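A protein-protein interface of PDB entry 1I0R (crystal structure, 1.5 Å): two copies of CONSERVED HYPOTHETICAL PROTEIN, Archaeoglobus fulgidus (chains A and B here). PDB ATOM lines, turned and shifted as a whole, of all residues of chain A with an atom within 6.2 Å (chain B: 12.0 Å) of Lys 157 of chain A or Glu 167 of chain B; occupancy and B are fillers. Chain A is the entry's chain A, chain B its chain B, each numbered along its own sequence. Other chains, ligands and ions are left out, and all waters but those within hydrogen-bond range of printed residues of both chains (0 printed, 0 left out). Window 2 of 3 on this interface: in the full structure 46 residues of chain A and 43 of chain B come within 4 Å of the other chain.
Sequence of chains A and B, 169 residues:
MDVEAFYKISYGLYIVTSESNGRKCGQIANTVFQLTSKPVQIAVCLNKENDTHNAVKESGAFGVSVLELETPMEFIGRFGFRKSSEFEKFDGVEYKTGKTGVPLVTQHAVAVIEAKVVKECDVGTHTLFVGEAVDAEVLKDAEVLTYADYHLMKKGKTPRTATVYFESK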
ATOM      1  N   LEU A 152      32.018   2.377  15.724  1.00  0.00           N
ATOM      2  CA  LEU A 152      30.600   2.661  15.834  1.00  0.00           C
ATOM      3  C   LEU A 152      30.521   4.101  16.335  1.00  0.00           C
ATOM      4  O   LEU A 152      29.647   4.865  15.918  1.00  0.00           O
ATOM      5  CB  LEU A 152      29.913   1.700  16.808  1.00  0.00           C
ATOM      6  CG  LEU A 152      29.873   0.231  16.371  1.00  0.00           C
ATOM      7  CD1 LEU A 152      29.114  -0.559  17.417  1.00  0.00           C
ATOM      8  CD2 LEU A 152      29.205   0.080  14.990  1.00  0.00           C
ATOM      9  N   MET A 153      31.455   4.485  17.206  1.00  0.00           N
ATOM     10  CA  MET A 153      31.468   5.852  17.718  1.00  0.00           C
ATOM     11  C   MET A 153      31.725   6.833  16.582  1.00  0.00           C
ATOM     12  O   MET A 153      31.098   7.893  16.522  1.00  0.00           O
ATOM     13  CB  MET A 153      32.542   6.028  18.793  1.00  0.00           C
ATOM     14  CG  MET A 153      32.261   5.281  20.084  1.00  0.00           C
ATOM     15  SD  MET A 153      33.693   5.398  21.185  1.00  0.00           S
ATOM     16  CE  MET A 153      33.495   7.096  21.814  1.00  0.00           C
ATOM     17  N   LYS A 154      32.651   6.496  15.687  1.00  0.00           N
ATOM     18  CA  LYS A 154      32.945   7.371  14.553  1.00  0.00           C
ATOM     19  C   LYS A 154      31.669   7.635  13.758  1.00  0.00           C
ATOM     20  O   LYS A 154      31.441   8.748  13.287  1.00  0.00           O
ATOM     21  CB  LYS A 154      33.988   6.739  13.620  1.00  0.00           C
ATOM     22  CG  LYS A 154      35.409   6.735  14.154  1.00  0.00           C
ATOM     23  CD  LYS A 154      36.391   6.181  13.114  1.00  0.00           C
ATOM     24  CE  LYS A 154      36.411   7.040  11.853  1.00  0.00           C
ATOM     25  NZ  LYS A 154      37.508   6.674  10.901  1.00  0.00           N
ATOM     26  N   LYS A 155      30.849   6.600  13.610  1.00  0.00           N
ATOM     27  CA  LYS A 155      29.598   6.706  12.868  1.00  0.00           C
ATOM     28  C   LYS A 155      28.498   7.414  13.659  1.00  0.00           C
ATOM     29  O   LYS A 155      27.353   7.482  13.211  1.00  0.00           O
ATOM     30  CB  LYS A 155      29.124   5.315  12.437  1.00  0.00           C
ATOM     31  CG  LYS A 155      30.000   4.656  11.370  1.00  0.00           C
ATOM     32  CD  LYS A 155      29.447   3.278  10.995  1.00  0.00           C
ATOM     33  CE  LYS A 155      30.213   2.626   9.845  1.00  0.00           C
ATOM     34  NZ  LYS A 155      31.633   2.297  10.177  1.00  0.00           N
ATOM     35  N   GLY A 156      28.838   7.929  14.836  1.00  0.00           N
ATOM     36  CA  GLY A 156      27.858   8.655  15.626  1.00  0.00           C
ATOM     37  C   GLY A 156      27.190   7.967  16.802  1.00  0.00           C
ATOM     38  O   GLY A 156      26.538   8.632  17.609  1.00  0.00           O
ATOM     39  N   LYS A 157      27.330   6.651  16.909  1.00  0.00           N
ATOM     40  CA  LYS A 157      26.718   5.924  18.015  1.00  0.00           C
ATOM     41  C   LYS A 157      27.395   6.326  19.329  1.00  0.00           C
ATOM     42  O   LYS A 157      28.470   6.926  19.334  1.00  0.00           O
ATOM     43  CB  LYS A 157      26.874   4.416  17.798  1.00  0.00           C
ATOM     44  CG  LYS A 157      26.502   3.946  16.402  1.00  0.00           C
ATOM     45  CD  LYS A 157      25.062   3.479  16.306  1.00  0.00           C
ATOM     46  CE  LYS A 157      24.882   2.125  16.976  1.00  0.00           C
ATOM     47  NZ  LYS A 157      23.506   1.578  16.770  1.00  0.00           N
ATOM     48  N   THR A 158      26.756   6.004  20.445  1.00  0.00           N
ATOM     49  CA  THR A 158      27.321   6.320  21.749  1.00  0.00           C
ATOM     50  C   THR A 158      26.947   5.198  22.721  1.00  0.00           C
ATOM     51  O   THR A 158      25.802   4.749  22.755  1.00  0.00           O
ATOM     52  CB  THR A 158      26.805   7.685  22.269  1.00  0.00           C
ATOM     53  OG1 THR A 158      27.591   8.097  23.394  1.00  0.00           O
ATOM     54  CG2 THR A 158      25.347   7.592  22.679  1.00  0.00           C
ATOM     55  N   PRO A 159      27.920   4.715  23.507  1.00  0.00           N
ATOM     56  CA  PRO A 159      27.687   3.637  24.476  1.00  0.00           C
ATOM     57  C   PRO A 159      26.655   4.024  25.529  1.00  0.00           C
ATOM     58  O   PRO A 159      26.568   5.187  25.917  1.00  0.00           O
ATOM     59  CB  PRO A 159      29.066   3.428  25.103  1.00  0.00           C
ATOM     60  CG  PRO A 159      30.017   3.940  24.058  1.00  0.00           C
ATOM     61  CD  PRO A 159      29.320   5.165  23.556  1.00  0.00           C
ATOM     62  N   ARG A 160      25.870   3.055  25.985  1.00  0.00           N
ATOM     63  CA  ARG A 160      24.884   3.331  27.018  1.00  0.00           C
ATOM     64  C   ARG A 160      25.007   2.346  28.169  1.00  0.00           C
ATOM     65  O   ARG A 160      24.993   1.132  27.966  1.00  0.00           O
ATOM     66  CB  ARG A 160      23.460   3.287  26.465  1.00  0.00           C
ATOM     67  CG  ARG A 160      22.437   3.662  27.527  1.00  0.00           C
ATOM     68  CD  ARG A 160      21.035   3.827  26.981  1.00  0.00           C
ATOM     69  NE  ARG A 160      20.112   4.227  28.042  1.00  0.00           N
ATOM     70  CZ  ARG A 160      18.798   4.362  27.883  1.00  0.00           C
ATOM     71  NH1 ARG A 160      18.246   4.129  26.701  1.00  0.00           N
ATOM     72  NH2 ARG A 160      18.037   4.714  28.912  1.00  0.00           N
ATOM     73  N   GLU B 143      28.685 -11.210  12.037  1.00  0.00           N
ATOM     74  CA  GLU B 143      29.470 -10.544  13.070  1.00  0.00           C
ATOM     75  C   GLU B 143      30.617 -11.482  13.427  1.00  0.00           C
ATOM     76  O   GLU B 143      30.492 -12.701  13.299  1.00  0.00           O
ATOM     77  CB  GLU B 143      28.618 -10.270  14.320  1.00  0.00           C
ATOM     78  CG  GLU B 143      27.473  -9.269  14.111  1.00  0.00           C
ATOM     79  CD  GLU B 143      27.927  -7.972  13.442  1.00  0.00           C
ATOM     80  OE1 GLU B 143      28.865  -7.321  13.958  1.00  0.00           O
ATOM     81  OE2 GLU B 143      27.342  -7.596  12.397  1.00  0.00           O
ATOM     82  N   ARG B 160      28.879 -10.371  25.006  1.00  0.00           N
ATOM     83  CA  ARG B 160      28.917  -8.942  25.281  1.00  0.00           C
ATOM     84  C   ARG B 160      27.617  -8.257  24.849  1.00  0.00           C
ATOM     85  O   ARG B 160      27.098  -7.387  25.552  1.00  0.00           O
ATOM     86  CB  ARG B 160      30.098  -8.304  24.551  1.00  0.00           C
ATOM     87  CG  ARG B 160      30.653  -7.065  25.237  1.00  0.00           C
ATOM     88  CD  ARG B 160      31.505  -6.260  24.276  1.00  0.00           C
ATOM     89  NE  ARG B 160      32.261  -5.204  24.943  1.00  0.00           N
ATOM     90  CZ  ARG B 160      32.654  -4.085  24.343  1.00  0.00           C
ATOM     91  NH1 ARG B 160      32.356  -3.879  23.069  1.00  0.00           N
ATOM     92  NH2 ARG B 160      33.350  -3.178  25.009  1.00  0.00           N
ATOM     93  N   THR B 161      27.099  -8.662  23.692  1.00  0.00           N
ATOM     94  CA  THR B 161      25.867  -8.102  23.137  1.00  0.00           C
ATOM     95  C   THR B 161      24.744  -7.935  24.162  1.00  0.00           C
ATOM     96  O   THR B 161      23.747  -7.259  23.899  1.00  0.00           O
ATOM     97  CB  THR B 161      25.340  -8.981  21.975  1.00  0.00           C
ATOM     98  OG1 THR B 161      24.095  -8.458  21.498  1.00  0.00           O
ATOM     99  CG2 THR B 161      25.134 -10.416  22.442  1.00  0.00           C
ATOM    100  N   THR B 163      25.174  -6.630  27.356  1.00  0.00           N
ATOM    101  CA  THR B 163      25.342  -5.443  28.195  1.00  0.00           C
ATOM    102  C   THR B 163      25.721  -4.166  27.448  1.00  0.00           C
ATOM    103  O   THR B 163      25.277  -3.077  27.811  1.00  0.00           O
ATOM    104  CB  THR B 163      26.399  -5.685  29.298  1.00  0.00           C
ATOM    105  OG1 THR B 163      27.593  -6.217  28.710  1.00  0.00           O
ATOM    106  CG2 THR B 163      25.868  -6.653  30.344  1.00  0.00           C
ATOM    107  N   VAL B 164      26.540  -4.296  26.411  1.00  0.00           N
ATOM    108  CA  VAL B 164      26.968  -3.130  25.648  1.00  0.00           C
ATOM    109  C   VAL B 164      25.931  -2.746  24.594  1.00  0.00           C
ATOM    110  O   VAL B 164      25.621  -3.528  23.695  1.00  0.00           O
ATOM    111  CB  VAL B 164      28.323  -3.385  24.956  1.00  0.00           C
ATOM    112  CG1 VAL B 164      28.830  -2.098  24.328  1.00  0.00           C
ATOM    113  CG2 VAL B 164      29.330  -3.916  25.965  1.00  0.00           C
ATOM    114  N   TYR B 165      25.408  -1.531  24.715  1.00  0.00           N
ATOM    115  CA  TYR B 165      24.401  -1.027  23.792  1.00  0.00           C
ATOM    116  C   TYR B 165      24.797   0.314  23.175  1.00  0.00           C
ATOM    117  O   TYR B 165      25.127   1.257  23.888  1.00  0.00           O
ATOM    118  CB  TYR B 165      23.064  -0.883  24.530  1.00  0.00           C
ATOM    119  CG  TYR B 165      21.967  -0.260  23.699  1.00  0.00           C
ATOM    120  CD1 TYR B 165      21.673  -0.745  22.428  1.00  0.00           C
ATOM    121  CD2 TYR B 165      21.229   0.821  24.182  1.00  0.00           C
ATOM    122  CE1 TYR B 165      20.677  -0.169  21.654  1.00  0.00           C
ATOM    123  CE2 TYR B 165      20.229   1.405  23.417  1.00  0.00           C
ATOM    124  CZ  TYR B 165      19.960   0.906  22.152  1.00  0.00           C
ATOM    125  OH  TYR B 165      18.983   1.486  21.378  1.00  0.00           O
ATOM    126  N   PHE B 166      24.765   0.393  21.848  1.00  0.00           N
ATOM    127  CA  PHE B 166      25.110   1.631  21.157  1.00  0.00           C
ATOM    128  C   PHE B 166      23.882   2.327  20.585  1.00  0.00           C
ATOM    129  O   PHE B 166      23.218   1.813  19.683  1.00  0.00           O
ATOM    130  CB  PHE B 166      26.118   1.377  20.030  1.00  0.00           C
ATOM    131  CG  PHE B 166      27.533   1.205  20.509  1.00  0.00           C
ATOM    132  CD1 PHE B 166      27.996  -0.036  20.930  1.00  0.00           C
ATOM    133  CD2 PHE B 166      28.396   2.295  20.561  1.00  0.00           C
ATOM    134  CE1 PHE B 166      29.302  -0.190  21.399  1.00  0.00           C
ATOM    135  CE2 PHE B 166      29.701   2.153  21.026  1.00  0.00           C
ATOM    136  CZ  PHE B 166      30.155   0.908  21.447  1.00  0.00           C
ATOM    137  N   GLU B 167      23.588   3.504  21.124  1.00  0.00           N
ATOM    138  CA  GLU B 167      22.454   4.297  20.681  1.00  0.00           C
ATOM    139  C   GLU B 167      22.976   5.525  19.937  1.00  0.00           C
ATOM    140  O   GLU B 167      24.096   5.971  20.180  1.00  0.00           O
ATOM    141  CB  GLU B 167      21.594   4.682  21.899  1.00  0.00           C
ATOM    142  CG  GLU B 167      21.207   6.156  22.043  1.00  0.00           C
ATOM    143  CD  GLU B 167      22.130   6.921  22.986  1.00  0.00           C
ATOM    144  OE1 GLU B 167      22.597   6.325  23.983  1.00  0.00           O
ATOM    145  OE2 GLU B 167      22.374   8.123  22.743  1.00  0.00           O
ATOM    146  N   SER B 168      22.176   6.057  19.016  1.00  0.00           N
ATOM    147  CA  SER B 168      22.588   7.228  18.243  1.00  0.00           C
ATOM    148  C   SER B 168      22.154   8.544  18.890  1.00  0.00           C
ATOM    149  O   SER B 168      21.456   8.494  19.926  1.00  0.00           O
ATOM    150  CB  SER B 168      22.024   7.144  16.820  1.00  0.00           C
ATOM    151  OG  SER B 168      20.614   7.033  16.844  1.00  0.00           O
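The side-chain amino group (NZ) of Lys 157 of chain A sits at hydrogen-bond distance from the backbone carbonyl oxygen (O) of Phe 166 of chain B (2.9 Å). The backbone NH (N) of Thr 158 of chain A lies within hydrogen-bond range of the backbone carbonyl oxygen (O) of Glu 167 of chain B, 2.7 Å away. O of Tyr 165 of chain B lies within hydrogen-bond range of N of Arg 160 of chain A (2.9 Å).
Printed residues of chain B that touch a printed residue of chain A: Tyr 165, Phe 166 and Glu 167. Hydrophobic or aromatic side chains of chain B that line the printed part of chain A: Phe 166.
Position printed for both chains: 160. Of the 9 pairs that touch across the chains among the printed residues, none has its exchanged pair printed and touching as well.
The backbone NH (N) of Lys 157 of chain A is in hydrogen-bond range of the backbone carbonyl oxygen (O) of Leu 152 of chain A, 3.1 Å away.
No residue of chain B comes within 4 Å of Met 153 of chain A. Lys 154 of chain A touches none of the printed residues of chain B. Lys 157 of chain A touches just these residues of chain B: Phe 166 (2.9 Å) and Glu 167 (3.4 Å). Printed residues of chain B within 4 Å of Thr 158 of chain A: Tyr 165 (3.7 Å), Phe 166 (3.6 Å) and Glu 167 (2.7 Å). Pro 159 of chain A touches just these residues of chain B: Tyr 165 (3.5 Å) and Phe 166 (3.5 Å). Printed residues of chain B within 4 Å of Arg 160 of chain A: Tyr 165. Arg 160 of chain B touches none of the printed residues of chain A. Printed residues of chain A within 4 Å of Tyr 165 of chain B: Thr 158, Pro 159 and Arg 160. Printed residues of chain A within 4 Å of Phe 166 of chain B: Leu 152, Lys 157, Thr 158 and Pro 159. Of the printed residues of chain A, Glu 167 of chain B touches Lys 157 (3.4 Å) and Thr 158 (2.7 Å). The nearest residue of chain B that does not touch Lys 157 of chain A is Ser 168 of chain B (4.3 Å). The nearest printed residue of chain B that does not touch Arg 160 of chain A is Glu 167 of chain B (4.02 Å).
Among the printed residues, merely in contact across the chains: Leu 152 of chain A with Phe 166 of chain B (3.7 Å), Lys 157 of chain A with Glu 167 of chain B (3.4 Å), Thr 158 of chain A with Tyr 165 of chain B (3.7 Å), Thr 158 of chain A with Phe 166 of chain B (3.6 Å), Pro 159 of chain A with Tyr 165 of chain B (3.5 Å) and Pro 159 of chain A with Phe 166 of chain B (3.5 Å).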
